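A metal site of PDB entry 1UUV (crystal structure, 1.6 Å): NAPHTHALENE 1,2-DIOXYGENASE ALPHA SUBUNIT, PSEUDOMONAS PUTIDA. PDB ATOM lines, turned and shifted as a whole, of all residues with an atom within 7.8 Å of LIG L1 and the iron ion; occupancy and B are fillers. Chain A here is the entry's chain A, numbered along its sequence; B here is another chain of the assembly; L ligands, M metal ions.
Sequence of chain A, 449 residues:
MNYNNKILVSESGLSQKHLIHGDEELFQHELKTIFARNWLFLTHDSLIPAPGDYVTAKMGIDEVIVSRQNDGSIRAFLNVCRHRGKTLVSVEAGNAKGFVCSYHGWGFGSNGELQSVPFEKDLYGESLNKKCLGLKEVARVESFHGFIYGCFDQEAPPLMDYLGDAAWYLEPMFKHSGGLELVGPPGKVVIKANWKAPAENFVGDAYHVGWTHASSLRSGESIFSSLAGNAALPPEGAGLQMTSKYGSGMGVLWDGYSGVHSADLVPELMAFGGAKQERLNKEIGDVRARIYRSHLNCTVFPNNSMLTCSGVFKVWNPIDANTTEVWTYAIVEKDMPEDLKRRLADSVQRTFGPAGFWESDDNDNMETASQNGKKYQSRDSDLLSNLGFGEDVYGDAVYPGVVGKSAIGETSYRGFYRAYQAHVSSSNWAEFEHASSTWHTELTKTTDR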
ATOM      1  N   ASN A 201      -2.872  11.058  -6.797  1.00  0.00           N
ATOM      2  CA  ASN A 201      -3.683  11.148  -7.998  1.00  0.00           C
ATOM      3  C   ASN A 201      -3.661   9.814  -8.722  1.00  0.00           C
ATOM      4  O   ASN A 201      -4.709   9.251  -9.087  1.00  0.00           O
ATOM      5  CB  ASN A 201      -3.169  12.282  -8.889  1.00  0.00           C
ATOM      6  CG  ASN A 201      -4.002  12.487 -10.155  1.00  0.00           C
ATOM      7  OD1 ASN A 201      -3.539  12.200 -11.250  1.00  0.00           O
ATOM      8  ND2 ASN A 201      -5.218  12.989  -9.995  1.00  0.00           N
ATOM      9  N   PHE A 202      -2.464   9.247  -8.880  1.00  0.00           N
ATOM     10  CA  PHE A 202      -2.333   7.977  -9.567  1.00  0.00           C
ATOM     11  C   PHE A 202      -2.824   6.767  -8.745  1.00  0.00           C
ATOM     12  O   PHE A 202      -3.242   5.761  -9.315  1.00  0.00           O
ATOM     13  CB  PHE A 202      -0.892   7.696  -9.980  1.00  0.00           C
ATOM     14  CG  PHE A 202      -0.494   8.314 -11.264  1.00  0.00           C
ATOM     15  CD1 PHE A 202      -0.485   9.689 -11.408  1.00  0.00           C
ATOM     16  CD2 PHE A 202      -0.147   7.547 -12.339  1.00  0.00           C
ATOM     17  CE1 PHE A 202      -0.168  10.274 -12.605  1.00  0.00           C
ATOM     18  CE2 PHE A 202       0.219   8.158 -13.555  1.00  0.00           C
ATOM     19  CZ  PHE A 202       0.188   9.529 -13.663  1.00  0.00           C
ATOM     20  N   ASP A 205      -7.284   8.104  -8.036  1.00  0.00           N
ATOM     21  CA  ASP A 205      -8.159   9.136  -8.545  1.00  0.00           C
ATOM     22  C   ASP A 205      -8.685   8.929  -9.959  1.00  0.00           C
ATOM     23  O   ASP A 205      -8.110   9.417 -10.937  1.00  0.00           O
ATOM     24  CB  ASP A 205      -7.437  10.483  -8.468  1.00  0.00           C
ATOM     25  CG  ASP A 205      -8.376  11.640  -8.650  1.00  0.00           C
ATOM     26  OD1 ASP A 205      -8.062  12.729  -8.110  1.00  0.00           O
ATOM     27  OD2 ASP A 205      -9.457  11.567  -9.287  1.00  0.00           O
ATOM     28  N   ALA A 206      -9.796   8.209 -10.080  1.00  0.00           N
ATOM     29  CA  ALA A 206     -10.465   8.156 -11.366  1.00  0.00           C
ATOM     30  C   ALA A 206     -11.495   9.277 -11.515  1.00  0.00           C
ATOM     31  O   ALA A 206     -11.898   9.566 -12.633  1.00  0.00           O
ATOM     32  CB  ALA A 206     -11.129   6.841 -11.574  1.00  0.00           C
ATOM     33  N   HIS A 208     -11.231  12.466 -11.302  1.00  0.00           N
ATOM     34  CA  HIS A 208     -10.750  13.651 -12.027  1.00  0.00           C
ATOM     35  C   HIS A 208     -10.691  13.517 -13.539  1.00  0.00           C
ATOM     36  O   HIS A 208     -10.652  14.512 -14.255  1.00  0.00           O
ATOM     37  CB  HIS A 208      -9.329  14.042 -11.533  1.00  0.00           C
ATOM     38  CG  HIS A 208      -8.215  13.289 -12.204  1.00  0.00           C
ATOM     39  ND1 HIS A 208      -8.000  11.940 -12.021  1.00  0.00           N
ATOM     40  CD2 HIS A 208      -7.237  13.716 -13.043  1.00  0.00           C
ATOM     41  CE1 HIS A 208      -6.959  11.555 -12.740  1.00  0.00           C
ATOM     42  NE2 HIS A 208      -6.490  12.615 -13.374  1.00  0.00           N
ATOM     43  N   VAL A 209     -10.700  12.277 -14.035  1.00  0.00           N
ATOM     44  CA  VAL A 209     -10.361  12.043 -15.430  1.00  0.00           C
ATOM     45  C   VAL A 209     -11.268  12.767 -16.405  1.00  0.00           C
ATOM     46  O   VAL A 209     -10.784  13.482 -17.282  1.00  0.00           O
ATOM     47  CB  VAL A 209     -10.243  10.548 -15.719  1.00  0.00           C
ATOM     48  CG1 VAL A 209     -10.107  10.304 -17.231  1.00  0.00           C
ATOM     49  CG2 VAL A 209      -9.031   9.960 -14.948  1.00  0.00           C
ATOM     50  N   GLY A 210     -12.570  12.635 -16.229  1.00  0.00           N
ATOM     51  CA  GLY A 210     -13.527  13.233 -17.138  1.00  0.00           C
ATOM     52  C   GLY A 210     -13.471  14.744 -17.190  1.00  0.00           C
ATOM     53  O   GLY A 210     -13.640  15.350 -18.255  1.00  0.00           O
ATOM     54  N   THR A 212     -10.751  16.951 -15.496  1.00  0.00           N
ATOM     55  CA  THR A 212      -9.386  17.449 -15.685  1.00  0.00           C
ATOM     56  C   THR A 212      -8.915  17.222 -17.096  1.00  0.00           C
ATOM     57  O   THR A 212      -8.332  18.110 -17.732  1.00  0.00           O
ATOM     58  CB  THR A 212      -8.423  16.733 -14.734  1.00  0.00           C
ATOM     59  OG1 THR A 212      -8.592  17.261 -13.412  1.00  0.00           O
ATOM     60  CG2 THR A 212      -6.972  17.047 -15.086  1.00  0.00           C
ATOM     61  N   HIS A 213      -9.202  16.031 -17.618  1.00  0.00           N
ATOM     62  CA  HIS A 213      -8.706  15.636 -18.924  1.00  0.00           C
ATOM     63  C   HIS A 213      -9.737  15.763 -20.034  1.00  0.00           C
ATOM     64  O   HIS A 213      -9.550  15.168 -21.102  1.00  0.00           O
ATOM     65  CB  HIS A 213      -8.128  14.205 -18.901  1.00  0.00           C
ATOM     66  CG  HIS A 213      -6.976  14.018 -17.939  1.00  0.00           C
ATOM     67  ND1 HIS A 213      -5.758  14.645 -18.100  1.00  0.00           N
ATOM     68  CD2 HIS A 213      -6.866  13.263 -16.825  1.00  0.00           C
ATOM     69  CE1 HIS A 213      -4.956  14.306 -17.110  1.00  0.00           C
ATOM     70  NE2 HIS A 213      -5.603  13.469 -16.322  1.00  0.00           N
ATOM     71  N   LEU A 217      -9.162  13.954 -23.625  1.00  0.00           N
ATOM     72  CA  LEU A 217     -10.090  12.911 -23.998  1.00  0.00           C
ATOM     73  C   LEU A 217     -10.721  13.259 -25.353  1.00  0.00           C
ATOM     74  O   LEU A 217     -10.693  12.437 -26.266  1.00  0.00           O
ATOM     75  CB  LEU A 217     -11.152  12.766 -22.930  1.00  0.00           C
ATOM     76  CG  LEU A 217     -10.605  12.132 -21.667  1.00  0.00           C
ATOM     77  CD1 LEU A 217     -11.555  12.363 -20.501  1.00  0.00           C
ATOM     78  CD2 LEU A 217     -10.342  10.640 -21.868  1.00  0.00           C
ATOM     79  N   PHE A 224     -11.062   5.778 -23.439  1.00  0.00           N
ATOM     80  CA  PHE A 224     -11.753   6.315 -22.272  1.00  0.00           C
ATOM     81  C   PHE A 224     -12.497   7.614 -22.554  1.00  0.00           C
ATOM     82  O   PHE A 224     -13.084   8.219 -21.649  1.00  0.00           O
ATOM     83  CB  PHE A 224     -10.727   6.554 -21.162  1.00  0.00           C
ATOM     84  CG  PHE A 224     -10.128   5.290 -20.616  1.00  0.00           C
ATOM     85  CD1 PHE A 224     -10.920   4.165 -20.415  1.00  0.00           C
ATOM     86  CD2 PHE A 224      -8.796   5.229 -20.289  1.00  0.00           C
ATOM     87  CE1 PHE A 224     -10.391   3.013 -19.910  1.00  0.00           C
ATOM     88  CE2 PHE A 224      -8.251   4.060 -19.776  1.00  0.00           C
ATOM     89  CZ  PHE A 224      -9.050   2.955 -19.581  1.00  0.00           C
ATOM     90  N   VAL A 260      -4.733   5.301 -22.440  1.00  0.00           N
ATOM     91  CA  VAL A 260      -4.801   6.692 -22.878  1.00  0.00           C
ATOM     92  C   VAL A 260      -4.364   6.874 -24.343  1.00  0.00           C
ATOM     93  O   VAL A 260      -4.380   8.017 -24.870  1.00  0.00           O
ATOM     94  CB  VAL A 260      -3.944   7.577 -21.961  1.00  0.00           C
ATOM     95  CG1 VAL A 260      -4.343   7.374 -20.477  1.00  0.00           C
ATOM     96  CG2 VAL A 260      -2.479   7.279 -22.189  1.00  0.00           C
ATOM     97  N   HIS A 295      -6.956  -1.753 -17.361  1.00  0.00           N
ATOM     98  CA  HIS A 295      -6.114  -0.599 -17.062  1.00  0.00           C
ATOM     99  C   HIS A 295      -5.998  -0.408 -15.548  1.00  0.00           C
ATOM    100  O   HIS A 295      -7.005  -0.166 -14.873  1.00  0.00           O
ATOM    101  CB  HIS A 295      -6.758   0.627 -17.684  1.00  0.00           C
ATOM    102  CG  HIS A 295      -5.859   1.808 -17.818  1.00  0.00           C
ATOM    103  ND1 HIS A 295      -5.858   2.856 -16.906  1.00  0.00           N
ATOM    104  CD2 HIS A 295      -4.960   2.136 -18.773  1.00  0.00           C
ATOM    105  CE1 HIS A 295      -4.992   3.767 -17.309  1.00  0.00           C
ATOM    106  NE2 HIS A 295      -4.414   3.347 -18.427  1.00  0.00           N
ATOM    107  N   ASN A 297      -4.378   1.864 -12.590  1.00  0.00           N
ATOM    108  CA  ASN A 297      -3.699   3.083 -12.156  1.00  0.00           C
ATOM    109  C   ASN A 297      -3.247   2.841 -10.730  1.00  0.00           C
ATOM    110  O   ASN A 297      -4.044   2.769  -9.813  1.00  0.00           O
ATOM    111  CB  ASN A 297      -4.589   4.323 -12.312  1.00  0.00           C
ATOM    112  CG  ASN A 297      -5.845   4.249 -11.515  1.00  0.00           C
ATOM    113  OD1 ASN A 297      -6.794   3.553 -11.883  1.00  0.00           O
ATOM    114  ND2 ASN A 297      -5.888   4.974 -10.389  1.00  0.00           N
ATOM    115  N   LEU A 307       0.545   3.285 -14.960  1.00  0.00           N
ATOM    116  CA  LEU A 307      -0.714   3.015 -15.625  1.00  0.00           C
ATOM    117  C   LEU A 307      -0.420   1.772 -16.464  1.00  0.00           C
ATOM    118  O   LEU A 307       0.247   1.899 -17.494  1.00  0.00           O
ATOM    119  CB  LEU A 307      -1.194   4.139 -16.526  1.00  0.00           C
ATOM    120  CG  LEU A 307      -1.407   5.509 -15.905  1.00  0.00           C
ATOM    121  CD1 LEU A 307      -1.935   6.495 -16.941  1.00  0.00           C
ATOM    122  CD2 LEU A 307      -2.357   5.436 -14.724  1.00  0.00           C
ATOM    123  N   PHE A 352       2.025  11.453 -21.509  1.00  0.00           N
ATOM    124  CA  PHE A 352       2.433  11.633 -20.114  1.00  0.00           C
ATOM    125  C   PHE A 352       3.860  12.076 -19.855  1.00  0.00           C
ATOM    126  O   PHE A 352       4.262  12.204 -18.703  1.00  0.00           O
ATOM    127  CB  PHE A 352       2.079  10.365 -19.304  1.00  0.00           C
ATOM    128  CG  PHE A 352       0.665  10.370 -18.855  1.00  0.00           C
ATOM    129  CD1 PHE A 352       0.309  11.001 -17.682  1.00  0.00           C
ATOM    130  CD2 PHE A 352      -0.326   9.819 -19.627  1.00  0.00           C
ATOM    131  CE1 PHE A 352      -1.010  11.073 -17.289  1.00  0.00           C
ATOM    132  CE2 PHE A 352      -1.652   9.873 -19.219  1.00  0.00           C
ATOM    133  CZ  PHE A 352      -1.989  10.492 -18.057  1.00  0.00           C
ATOM    134  N   TRP A 358      -1.759  15.037 -21.742  1.00  0.00           N
ATOM    135  CA  TRP A 358      -2.585  14.645 -20.589  1.00  0.00           C
ATOM    136  C   TRP A 358      -1.931  15.133 -19.287  1.00  0.00           C
ATOM    137  O   TRP A 358      -2.587  15.719 -18.435  1.00  0.00           O
ATOM    138  CB  TRP A 358      -2.777  13.136 -20.467  1.00  0.00           C
ATOM    139  CG  TRP A 358      -3.593  12.468 -21.531  1.00  0.00           C
ATOM    140  CD1 TRP A 358      -3.335  12.413 -22.888  1.00  0.00           C
ATOM    141  CD2 TRP A 358      -4.747  11.658 -21.317  1.00  0.00           C
ATOM    142  NE1 TRP A 358      -4.293  11.655 -23.512  1.00  0.00           N
ATOM    143  CE2 TRP A 358      -5.179  11.192 -22.570  1.00  0.00           C
ATOM    144  CE3 TRP A 358      -5.489  11.307 -20.175  1.00  0.00           C
ATOM    145  CZ2 TRP A 358      -6.311  10.380 -22.728  1.00  0.00           C
ATOM    146  CZ3 TRP A 358      -6.603  10.502 -20.329  1.00  0.00           C
ATOM    147  CH2 TRP A 358      -7.005  10.050 -21.586  1.00  0.00           C
ATOM    148  N   GLU A 359      -0.635  14.868 -19.129  1.00  0.00           N
ATOM    149  CA  GLU A 359       0.090  15.288 -17.931  1.00  0.00           C
ATOM    150  C   GLU A 359      -0.046  16.815 -17.729  1.00  0.00           C
ATOM    151  O   GLU A 359      -0.175  17.288 -16.594  1.00  0.00           O
ATOM    152  CB  GLU A 359       1.576  14.873 -18.031  1.00  0.00           C
ATOM    153  CG  GLU A 359       2.450  15.207 -16.798  1.00  0.00           C
ATOM    154  CD  GLU A 359       2.688  14.068 -15.811  1.00  0.00           C
ATOM    155  OE1 GLU A 359       1.861  13.125 -15.702  1.00  0.00           O
ATOM    156  OE2 GLU A 359       3.711  14.150 -15.074  1.00  0.00           O
ATOM    157  N   ASP A 361      -2.572  18.649 -18.262  1.00  0.00           N
ATOM    158  CA  ASP A 361      -3.876  18.947 -17.696  1.00  0.00           C
ATOM    159  C   ASP A 361      -3.818  18.899 -16.177  1.00  0.00           C
ATOM    160  O   ASP A 361      -4.601  19.568 -15.515  1.00  0.00           O
ATOM    161  CB  ASP A 361      -4.946  17.932 -18.128  1.00  0.00           C
ATOM    162  CG  ASP A 361      -5.161  17.872 -19.628  1.00  0.00           C
ATOM    163  OD1 ASP A 361      -5.552  16.782 -20.114  1.00  0.00           O
ATOM    164  OD2 ASP A 361      -5.002  18.844 -20.400  1.00  0.00           O
ATOM    165  N   ASP A 362      -2.903  18.102 -15.635  1.00  0.00           N
ATOM    166  CA  ASP A 362      -2.847  17.858 -14.198  1.00  0.00           C
ATOM    167  C   ASP A 362      -1.966  18.841 -13.483  1.00  0.00           C
ATOM    168  O   ASP A 362      -2.039  18.941 -12.261  1.00  0.00           O
ATOM    169  CB  ASP A 362      -2.240  16.480 -13.889  1.00  0.00           C
ATOM    170  CG  ASP A 362      -3.116  15.321 -14.286  1.00  0.00           C
ATOM    171  OD1 ASP A 362      -2.631  14.479 -15.085  1.00  0.00           O
ATOM    172  OD2 ASP A 362      -4.231  15.084 -13.796  1.00  0.00           O
ATOM    173  N   ASN A 363      -1.103  19.552 -14.218  1.00  0.00           N
ATOM    174  CA  ASN A 363      -0.088  20.451 -13.614  1.00  0.00           C
ATOM    175  C   ASN A 363      -0.645  21.379 -12.582  1.00  0.00           C
ATOM    176  O   ASN A 363      -0.181  21.413 -11.437  1.00  0.00           O
ATOM    177  CB  ASN A 363       0.555  21.355 -14.676  1.00  0.00           C
ATOM    178  CG  ASN A 363       1.791  20.754 -15.327  1.00  0.00           C
ATOM    179  OD1 ASN A 363       2.439  21.405 -16.183  1.00  0.00           O
ATOM    180  ND2 ASN A 363       2.136  19.522 -14.944  1.00  0.00           N
ATOM    181  N   ASN A 365      -3.463  21.528 -11.098  1.00  0.00           N
ATOM    182  CA  ASN A 365      -4.141  20.857 -10.001  1.00  0.00           C
ATOM    183  C   ASN A 365      -3.146  20.505  -8.911  1.00  0.00           C
ATOM    184  O   ASN A 365      -3.377  20.802  -7.738  1.00  0.00           O
ATOM    185  CB  ASN A 365      -4.836  19.578 -10.452  1.00  0.00           C
ATOM    186  CG  ASN A 365      -6.010  19.826 -11.380  1.00  0.00           C
ATOM    187  OD1 ASN A 365      -6.626  20.876 -11.370  1.00  0.00           O
ATOM    188  ND2 ASN A 365      -6.319  18.828 -12.176  1.00  0.00           N
ATOM    189  N   MET A 366      -2.078  19.826  -9.288  1.00  0.00           N
ATOM    190  CA  MET A 366      -1.065  19.367  -8.338  1.00  0.00           C
ATOM    191  C   MET A 366      -0.299  20.519  -7.715  1.00  0.00           C
ATOM    192  O   MET A 366      -0.034  20.551  -6.508  1.00  0.00           O
ATOM    193  CB  MET A 366      -0.054  18.469  -9.016  1.00  0.00           C
ATOM    194  CG  MET A 366      -0.625  17.349  -9.849  1.00  0.00           C
ATOM    195  SD  MET A 366      -1.071  16.004  -8.870  1.00  0.00           S
ATOM    196  CE  MET A 366      -2.751  16.354  -8.505  1.00  0.00           C
ATOM    197  N   TYR B 103     -10.347  20.406 -11.050  1.00  0.00           N
ATOM    198  CA  TYR B 103      -9.788  19.119 -10.691  1.00  0.00           C
ATOM    199  C   TYR B 103     -10.855  18.031 -10.830  1.00  0.00           C
ATOM    200  O   TYR B 103     -10.782  17.208 -11.750  1.00  0.00           O
ATOM    201  CB  TYR B 103      -9.181  19.187  -9.294  1.00  0.00           C
ATOM    202  CG  TYR B 103      -8.156  18.112  -8.947  1.00  0.00           C
ATOM    203  CD1 TYR B 103      -7.403  18.221  -7.805  1.00  0.00           C
ATOM    204  CD2 TYR B 103      -7.961  17.019  -9.758  1.00  0.00           C
ATOM    205  CE1 TYR B 103      -6.455  17.238  -7.473  1.00  0.00           C
ATOM    206  CE2 TYR B 103      -7.029  16.017  -9.422  1.00  0.00           C
ATOM    207  CZ  TYR B 103      -6.289  16.131  -8.280  1.00  0.00           C
ATOM    208  OH  TYR B 103      -5.382  15.144  -7.964  1.00  0.00           O
HETATM  209  N1  LIG L   1      -4.875  11.212 -15.292  1.00  0.00           N
HETATM  210  O1  LIG L   1      -5.178  10.342 -16.158  1.00  0.00           O
HETATM  211  N1  LG2 L   2      -5.811   7.819 -12.379  1.00  0.00           N
HETATM  212  C1  LG2 L   2      -4.692   8.598 -12.625  1.00  0.00           C
HETATM  213  C2  LG2 L   2      -4.395   8.582 -13.979  1.00  0.00           C
HETATM  214  C3  LG2 L   2      -5.536   7.411 -15.890  1.00  0.00           C
HETATM  215  C4  LG2 L   2      -6.578   6.575 -16.221  1.00  0.00           C
HETATM  216  C5  LG2 L   2      -7.441   6.092 -15.240  1.00  0.00           C
HETATM  217  C6  LG2 L   2      -7.328   6.429 -13.897  1.00  0.00           C
HETATM  218  C7  LG2 L   2      -6.298   7.270 -13.514  1.00  0.00           C
HETATM  219  C8  LG2 L   2      -5.389   7.755 -14.562  1.00  0.00           C
HETATM  220 FE    FE M   1      -4.724  12.806 -14.691  1.00  0.00          FE
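The iron ion is bound by a nitrogen (N1) of LIG L1. A ring nitrogen (NE2) of His 213 binds the iron ion, 2.0 Å away. The iron ion is bound by NE2 of His 208 (2.2 Å). The side-chain carboxylate (OD2) of Asp 362 is bound to the iron ion (2.5 Å). The iron ion has four donor atoms within binding distance. Slightly farther from the iron ion lies the side-chain carboxylate (OD1) of Asp 362 (2.7 Å).
A nitrogen (N1) of LG2 L2 sits at hydrogen-bond distance from the backbone carbonyl oxygen (O) of Asp 205 (3.1 Å). A nitrogen (N1) of LG2 L2 sits close to the side-chain amide nitrogen (ND2) of Asn 297, 3.5 Å away.
Merely in contact with LIG L1: Phe 352 (3.7 Å). Hydrophobic or aromatic side chains within 4 Å of LIG L1: His 208, His 213 and Phe 352. The nearest printed residue that does not touch LIG L1 is Val 209 (4.1 Å).
The side-chain amide nitrogen (ND2) of Asn 201 sits at hydrogen-bond distance from the side-chain carboxylate (OD1) of Asp 205. ND2 of Asn 201 is in hydrogen-bond range of OH of Tyr 103 of chain B (3.0 Å). A ring nitrogen (ND1) of His 208 is in hydrogen-bond range of the backbone carbonyl oxygen of Asp 205 (2.7 Å). The side-chain carboxylate (OD1) of Asp 361 sits at hydrogen-bond distance from a ring nitrogen (ND1) of His 213 (2.9 Å). O of Trp 358 lies close to ND1 of His 213, at 3.4 Å.
Residues that only touch the iron ion: Asn 201.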
